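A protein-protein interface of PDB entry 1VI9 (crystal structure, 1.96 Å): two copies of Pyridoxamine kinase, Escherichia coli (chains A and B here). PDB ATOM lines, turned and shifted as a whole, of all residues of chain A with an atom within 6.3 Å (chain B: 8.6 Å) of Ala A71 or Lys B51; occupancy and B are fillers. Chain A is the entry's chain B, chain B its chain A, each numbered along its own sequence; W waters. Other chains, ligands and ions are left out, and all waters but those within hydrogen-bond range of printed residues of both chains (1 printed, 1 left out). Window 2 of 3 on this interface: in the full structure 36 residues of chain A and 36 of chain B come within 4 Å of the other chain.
Water W1 lies within hydrogen-bond range of the side-chain hydroxyl of Tyr B49 (2.6 Å) and the side-chain amino group of Lys A74 (3.3 Å).
Hydrophobic or aromatic side chains of chain B within 4 Å of the printed part of chain A: Tyr B49.
Hydrophobic or aromatic side chains of chain A that line the printed part of chain B: Ile A69 and Ile A72.
Among the printed residues, 8 pairs touch across the chains.
Among the printed residues, no Asp or Glu carboxylate lies within 4 Å of a Lys or Arg side-chain nitrogen of the other chain.
Among the printed residues, pairs that only touch across the chains: Ile A72 with Tyr B49, Gly A68 with Asn B45, Gly A68 with Thr B53, Gly A68 with Ser B44, Ile A72 with Asn B45, Ile A69 with Ser B44 and Ile A72 with Lys B51.
The side-chain amino group (NZ) of Lys B51 sits at hydrogen-bond distance from the backbone carbonyl oxygen (O) of Ala A71 (3.4 Å).
O of Lys B51 lies within hydrogen-bond range of ND2 of Asn B45 (2.7 Å).
The backbone carbonyl oxygen (O) of Thr B53 lies within hydrogen-bond range of the backbone NH (N) of Ser B44 (2.9 Å).
OG of Ser B44 sits at hydrogen-bond distance from OD1 of Asn B45, 2.7 Å away.
O of Ile A69 sits at hydrogen-bond distance from N of Lys A74 (3.2 Å).
Of the printed residues of chain B, Gly A68 touches Ser B44, Asn B45 and Thr B53.
No residue of chain B comes within 4 Å of Ala A70.
Of chain B, only Lys B51 comes within 4 Å of Ala A71.
Of the printed residues of chain B, Ile A72 touches Asn B45 (3.7 Å), Tyr B49 (3.5 Å) and Lys B51 (3.7 Å).
Printed residues of chain A within 4 Å of Ser B44: Gly A68 (3.7 Å) and Ile A69 (3.7 Å).
Of the printed residues of chain A, Tyr B49 touches Ile A72 (3.5 Å).
Lys B51 touches two residues of chain A.
Printed residues of chain A within 4 Å of Thr B53: Gly A68 (3.6 Å).
Gly B54 touches none of the printed residues of chain A.
The nearest residue of chain B that does not touch Ala A71 is Asn B45 (6.1 Å).
The nearest residue of chain A that does not touch Lys B51 is Gly A68 (5.8 Å).
The nearest printed residue of chain B that does not touch Gly A68 is Trp B52 (5.2 Å).
No position is printed for both chains.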
ATOM      1  N   VAL A  66     -10.821 -11.497  11.892  1.00  0.00           N
ATOM      2  CA  VAL A  66      -9.542 -11.972  12.406  1.00  0.00           C
ATOM      3  C   VAL A  66      -8.720 -12.675  11.337  1.00  0.00           C
ATOM      4  O   VAL A  66      -7.497 -12.562  11.266  1.00  0.00           O
ATOM      5  CB  VAL A  66      -9.742 -12.785  13.689  1.00  0.00           C
ATOM      6  CG1 VAL A  66      -8.451 -13.435  14.159  1.00  0.00           C
ATOM      7  CG2 VAL A  66     -10.282 -11.838  14.797  1.00  0.00           C
ATOM      8  N   GLN A  67      -9.369 -13.408  10.437  1.00  0.00           N
ATOM      9  CA  GLN A  67      -8.668 -14.081   9.322  1.00  0.00           C
ATOM     10  C   GLN A  67      -8.031 -13.022   8.439  1.00  0.00           C
ATOM     11  O   GLN A  67      -6.939 -13.163   7.889  1.00  0.00           O
ATOM     12  CB  GLN A  67      -9.720 -14.861   8.548  1.00  0.00           C
ATOM     13  CG  GLN A  67     -10.044 -16.272   8.887  1.00  0.00           C
ATOM     14  CD  GLN A  67      -9.384 -16.820  10.136  1.00  0.00           C
ATOM     15  OE1 GLN A  67      -9.960 -16.730  11.229  1.00  0.00           O
ATOM     16  NE2 GLN A  67      -8.164 -17.328   9.942  1.00  0.00           N
ATOM     17  N   GLY A  68      -8.747 -11.882   8.248  1.00  0.00           N
ATOM     18  CA  GLY A  68      -8.174 -10.811   7.432  1.00  0.00           C
ATOM     19  C   GLY A  68      -6.929 -10.231   8.078  1.00  0.00           C
ATOM     20  O   GLY A  68      -5.959  -9.908   7.408  1.00  0.00           O
ATOM     21  N   ILE A  69      -6.924 -10.057   9.410  1.00  0.00           N
ATOM     22  CA  ILE A  69      -5.732  -9.525  10.079  1.00  0.00           C
ATOM     23  C   ILE A  69      -4.646 -10.595  10.016  1.00  0.00           C
ATOM     24  O   ILE A  69      -3.457 -10.258   9.955  1.00  0.00           O
ATOM     25  CB  ILE A  69      -6.028  -9.120  11.533  1.00  0.00           C
ATOM     26  CG1 ILE A  69      -7.093  -8.023  11.532  1.00  0.00           C
ATOM     27  CG2 ILE A  69      -4.753  -8.657  12.256  1.00  0.00           C
ATOM     28  CD1 ILE A  69      -7.783  -7.794  12.851  1.00  0.00           C
ATOM     29  N   ALA A  70      -5.034 -11.873  10.068  1.00  0.00           N
ATOM     30  CA  ALA A  70      -4.000 -12.937   9.948  1.00  0.00           C
ATOM     31  C   ALA A  70      -3.447 -12.912   8.530  1.00  0.00           C
ATOM     32  O   ALA A  70      -2.227 -12.956   8.306  1.00  0.00           O
ATOM     33  CB  ALA A  70      -4.554 -14.277  10.352  1.00  0.00           C
ATOM     34  N   ALA A  71      -4.304 -12.588   7.552  1.00  0.00           N
ATOM     35  CA  ALA A  71      -3.895 -12.491   6.156  1.00  0.00           C
ATOM     36  C   ALA A  71      -2.860 -11.416   5.884  1.00  0.00           C
ATOM     37  O   ALA A  71      -1.999 -11.619   5.031  1.00  0.00           O
ATOM     38  CB  ALA A  71      -5.081 -12.324   5.202  1.00  0.00           C
ATOM     39  N   ILE A  72      -2.839 -10.298   6.623  1.00  0.00           N
ATOM     40  CA  ILE A  72      -1.820  -9.287   6.392  1.00  0.00           C
ATOM     41  C   ILE A  72      -0.640  -9.479   7.342  1.00  0.00           C
ATOM     42  O   ILE A  72       0.227  -8.633   7.420  1.00  0.00           O
ATOM     43  CB  ILE A  72      -2.350  -7.849   6.443  1.00  0.00           C
ATOM     44  CG1 ILE A  72      -3.213  -7.632   7.694  1.00  0.00           C
ATOM     45  CG2 ILE A  72      -3.147  -7.578   5.162  1.00  0.00           C
ATOM     46  CD1 ILE A  72      -3.495  -6.194   8.038  1.00  0.00           C
ATOM     47  N   ASP A  73      -0.610 -10.604   8.039  1.00  0.00           N
ATOM     48  CA  ASP A  73       0.457 -10.996   8.960  1.00  0.00           C
ATOM     49  C   ASP A  73       0.676 -10.011  10.074  1.00  0.00           C
ATOM     50  O   ASP A  73       1.810  -9.646  10.385  1.00  0.00           O
ATOM     51  CB  ASP A  73       1.761 -11.205   8.180  1.00  0.00           C
ATOM     52  CG  ASP A  73       2.726 -12.152   8.869  1.00  0.00           C
ATOM     53  OD1 ASP A  73       2.325 -12.901   9.778  1.00  0.00           O
ATOM     54  OD2 ASP A  73       3.915 -12.110   8.507  1.00  0.00           O
ATOM     55  N   LYS A  74      -0.417  -9.571  10.709  1.00  0.00           N
ATOM     56  CA  LYS A  74      -0.279  -8.596  11.785  1.00  0.00           C
ATOM     57  C   LYS A  74      -0.849  -9.153  13.072  1.00  0.00           C
ATOM     58  O   LYS A  74      -0.731  -8.522  14.121  1.00  0.00           O
ATOM     59  CB  LYS A  74      -1.004  -7.265  11.425  1.00  0.00           C
ATOM     60  CG  LYS A  74      -0.304  -6.501  10.309  1.00  0.00           C
ATOM     61  CD  LYS A  74       1.065  -5.997  10.731  1.00  0.00           C
ATOM     62  CE  LYS A  74       1.749  -5.276   9.587  1.00  0.00           C
ATOM     63  NZ  LYS A  74       2.677  -4.213  10.074  1.00  0.00           N
ATOM     64  N   PHE B  43     -14.427  -3.637   8.112  1.00  0.00           N
ATOM     65  CA  PHE B  43     -13.410  -4.371   7.386  1.00  0.00           C
ATOM     66  C   PHE B  43     -12.219  -4.709   8.297  1.00  0.00           C
ATOM     67  O   PHE B  43     -11.878  -3.966   9.244  1.00  0.00           O
ATOM     68  CB  PHE B  43     -12.928  -3.494   6.228  1.00  0.00           C
ATOM     69  CG  PHE B  43     -13.794  -3.463   5.001  1.00  0.00           C
ATOM     70  CD1 PHE B  43     -15.046  -4.044   4.956  1.00  0.00           C
ATOM     71  CD2 PHE B  43     -13.319  -2.822   3.857  1.00  0.00           C
ATOM     72  CE1 PHE B  43     -15.837  -3.981   3.822  1.00  0.00           C
ATOM     73  CE2 PHE B  43     -14.100  -2.779   2.709  1.00  0.00           C
ATOM     74  CZ  PHE B  43     -15.356  -3.343   2.707  1.00  0.00           C
ATOM     75  N   SER B  44     -11.506  -5.758   7.957  1.00  0.00           N
ATOM     76  CA  SER B  44     -10.367  -6.247   8.709  1.00  0.00           C
ATOM     77  C   SER B  44      -9.215  -5.236   8.733  1.00  0.00           C
ATOM     78  O   SER B  44      -8.581  -5.087   9.777  1.00  0.00           O
ATOM     79  CB  SER B  44      -9.854  -7.585   8.131  1.00  0.00           C
ATOM     80  OG  SER B  44      -9.305  -7.353   6.812  1.00  0.00           O
ATOM     81  N   ASN B  45      -9.013  -4.553   7.631  1.00  0.00           N
ATOM     82  CA  ASN B  45      -8.009  -3.606   7.300  1.00  0.00           C
ATOM     83  C   ASN B  45      -8.429  -2.823   6.042  1.00  0.00           C
ATOM     84  O   ASN B  45      -9.426  -3.171   5.403  1.00  0.00           O
ATOM     85  CB  ASN B  45      -6.627  -4.257   7.046  1.00  0.00           C
ATOM     86  CG  ASN B  45      -6.682  -5.385   6.030  1.00  0.00           C
ATOM     87  OD1 ASN B  45      -6.787  -6.583   6.399  1.00  0.00           O
ATOM     88  ND2 ASN B  45      -6.639  -5.045   4.755  1.00  0.00           N
ATOM     89  N   HIS B  46      -7.702  -1.750   5.748  1.00  0.00           N
ATOM     90  CA  HIS B  46      -8.129  -0.945   4.587  1.00  0.00           C
ATOM     91  C   HIS B  46      -7.782  -1.670   3.279  1.00  0.00           C
ATOM     92  O   HIS B  46      -6.968  -2.593   3.218  1.00  0.00           O
ATOM     93  CB  HIS B  46      -7.640   0.486   4.700  1.00  0.00           C
ATOM     94  CG  HIS B  46      -6.166   0.675   4.548  1.00  0.00           C
ATOM     95  ND1 HIS B  46      -5.522   0.408   3.336  1.00  0.00           N
ATOM     96  CD2 HIS B  46      -5.195   1.065   5.405  1.00  0.00           C
ATOM     97  CE1 HIS B  46      -4.235   0.625   3.489  1.00  0.00           C
ATOM     98  NE2 HIS B  46      -4.001   1.027   4.733  1.00  0.00           N
ATOM     99  N   THR B  47      -8.526  -1.345   2.244  1.00  0.00           N
ATOM    100  CA  THR B  47      -8.460  -1.888   0.916  1.00  0.00           C
ATOM    101  C   THR B  47      -7.181  -1.650   0.156  1.00  0.00           C
ATOM    102  O   THR B  47      -6.889  -2.436  -0.778  1.00  0.00           O
ATOM    103  CB  THR B  47      -9.652  -1.414   0.039  1.00  0.00           C
ATOM    104  OG1 THR B  47      -9.494  -0.018  -0.192  1.00  0.00           O
ATOM    105  CG2 THR B  47     -10.987  -1.649   0.713  1.00  0.00           C
ATOM    106  N   GLN B  48      -6.299  -0.729   0.527  1.00  0.00           N
ATOM    107  CA  GLN B  48      -5.056  -0.496  -0.166  1.00  0.00           C
ATOM    108  C   GLN B  48      -4.015  -1.581   0.105  1.00  0.00           C
ATOM    109  O   GLN B  48      -2.934  -1.603  -0.514  1.00  0.00           O
ATOM    110  CB  GLN B  48      -4.461   0.890   0.055  1.00  0.00           C
ATOM    111  CG  GLN B  48      -5.138   1.997  -0.743  1.00  0.00           C
ATOM    112  CD  GLN B  48      -5.282   1.675  -2.219  1.00  0.00           C
ATOM    113  OE1 GLN B  48      -4.352   1.849  -3.026  1.00  0.00           O
ATOM    114  NE2 GLN B  48      -6.470   1.185  -2.578  1.00  0.00           N
ATOM    115  N   TYR B  49      -4.293  -2.460   1.070  1.00  0.00           N
ATOM    116  CA  TYR B  49      -3.415  -3.610   1.288  1.00  0.00           C
ATOM    117  C   TYR B  49      -3.611  -4.565   0.090  1.00  0.00           C
ATOM    118  O   TYR B  49      -2.797  -5.468  -0.115  1.00  0.00           O
ATOM    119  CB  TYR B  49      -3.830  -4.415   2.522  1.00  0.00           C
ATOM    120  CG  TYR B  49      -3.314  -3.824   3.822  1.00  0.00           C
ATOM    121  CD1 TYR B  49      -2.147  -4.321   4.383  1.00  0.00           C
ATOM    122  CD2 TYR B  49      -3.983  -2.790   4.455  1.00  0.00           C
ATOM    123  CE1 TYR B  49      -1.673  -3.807   5.583  1.00  0.00           C
ATOM    124  CE2 TYR B  49      -3.523  -2.284   5.664  1.00  0.00           C
ATOM    125  CZ  TYR B  49      -2.367  -2.785   6.205  1.00  0.00           C
ATOM    126  OH  TYR B  49      -1.869  -2.306   7.394  1.00  0.00           O
ATOM    127  N   GLY B  50      -4.760  -4.469  -0.565  1.00  0.00           N
ATOM    128  CA  GLY B  50      -5.082  -5.303  -1.728  1.00  0.00           C
ATOM    129  C   GLY B  50      -5.776  -6.583  -1.285  1.00  0.00           C
ATOM    130  O   GLY B  50      -6.085  -7.471  -2.096  1.00  0.00           O
ATOM    131  N   LYS B  51      -6.018  -6.671   0.031  1.00  0.00           N
ATOM    132  CA  LYS B  51      -6.691  -7.852   0.583  1.00  0.00           C
ATOM    133  C   LYS B  51      -7.399  -7.470   1.885  1.00  0.00           C
ATOM    134  O   LYS B  51      -6.834  -6.653   2.603  1.00  0.00           O
ATOM    135  CB  LYS B  51      -5.667  -8.970   0.827  1.00  0.00           C
ATOM    136  CG  LYS B  51      -4.680  -8.650   1.933  1.00  0.00           C
ATOM    137  CD  LYS B  51      -3.293  -9.187   1.623  1.00  0.00           C
ATOM    138  CE  LYS B  51      -3.236 -10.673   1.939  1.00  0.00           C
ATOM    139  NZ  LYS B  51      -1.877 -11.207   1.658  1.00  0.00           N
ATOM    140  N   TRP B  52      -8.607  -7.941   2.133  1.00  0.00           N
ATOM    141  CA  TRP B  52      -9.335  -7.589   3.365  1.00  0.00           C
ATOM    142  C   TRP B  52     -10.572  -8.450   3.510  1.00  0.00           C
ATOM    143  O   TRP B  52     -11.032  -9.024   2.509  1.00  0.00           O
ATOM    144  CB  TRP B  52      -9.801  -6.115   3.300  1.00  0.00           C
ATOM    145  CG  TRP B  52     -10.778  -5.862   2.179  1.00  0.00           C
ATOM    146  CD1 TRP B  52     -12.143  -5.946   2.253  1.00  0.00           C
ATOM    147  CD2 TRP B  52     -10.472  -5.507   0.826  1.00  0.00           C
ATOM    148  NE1 TRP B  52     -12.700  -5.658   1.029  1.00  0.00           N
ATOM    149  CE2 TRP B  52     -11.699  -5.380   0.140  1.00  0.00           C
ATOM    150  CE3 TRP B  52      -9.289  -5.269   0.121  1.00  0.00           C
ATOM    151  CZ2 TRP B  52     -11.762  -5.038  -1.212  1.00  0.00           C
ATOM    152  CZ3 TRP B  52      -9.342  -4.937  -1.218  1.00  0.00           C
ATOM    153  CH2 TRP B  52     -10.583  -4.823  -1.873  1.00  0.00           C
ATOM    154  N   THR B  53     -11.126  -8.558   4.708  1.00  0.00           N
ATOM    155  CA  THR B  53     -12.359  -9.298   4.935  1.00  0.00           C
ATOM    156  C   THR B  53     -13.329  -8.309   5.597  1.00  0.00           C
ATOM    157  O   THR B  53     -12.906  -7.186   5.866  1.00  0.00           O
ATOM    158  CB  THR B  53     -12.219 -10.492   5.879  1.00  0.00           C
ATOM    159  OG1 THR B  53     -11.648  -9.999   7.110  1.00  0.00           O
ATOM    160  CG2 THR B  53     -11.292 -11.538   5.241  1.00  0.00           C
ATOM    161  N   GLY B  54     -14.540  -8.751   5.893  1.00  0.00           N
ATOM    162  CA  GLY B  54     -15.484  -7.833   6.516  1.00  0.00           C
ATOM    163  C   GLY B  54     -16.751  -7.677   5.687  1.00  0.00           C
ATOM    164  O   GLY B  54     -16.946  -8.295   4.646  1.00  0.00           O
ATOM    165  N   ARG B 219       4.709   2.529  -0.800  1.00  0.00           N
ATOM    166  CA  ARG B 219       3.688   2.084   0.172  1.00  0.00           C
ATOM    167  C   ARG B 219       3.154   3.310   0.894  1.00  0.00           C
ATOM    168  O   ARG B 219       3.546   3.557   2.022  1.00  0.00           O
ATOM    169  CB  ARG B 219       4.301   1.060   1.105  1.00  0.00           C
ATOM    170  CG  ARG B 219       4.127  -0.370   0.599  1.00  0.00           C
ATOM    171  CD  ARG B 219       3.975  -1.304   1.781  1.00  0.00           C
ATOM    172  NE  ARG B 219       2.608  -1.803   1.926  1.00  0.00           N
ATOM    173  CZ  ARG B 219       2.267  -2.578   2.959  1.00  0.00           C
ATOM    174  NH1 ARG B 219       3.206  -2.880   3.848  1.00  0.00           N
ATOM    175  NH2 ARG B 219       1.043  -3.067   3.045  1.00  0.00           N
HETATM  176  O   HOH W   1       0.681  -2.549   7.978  1.00  0.00           O
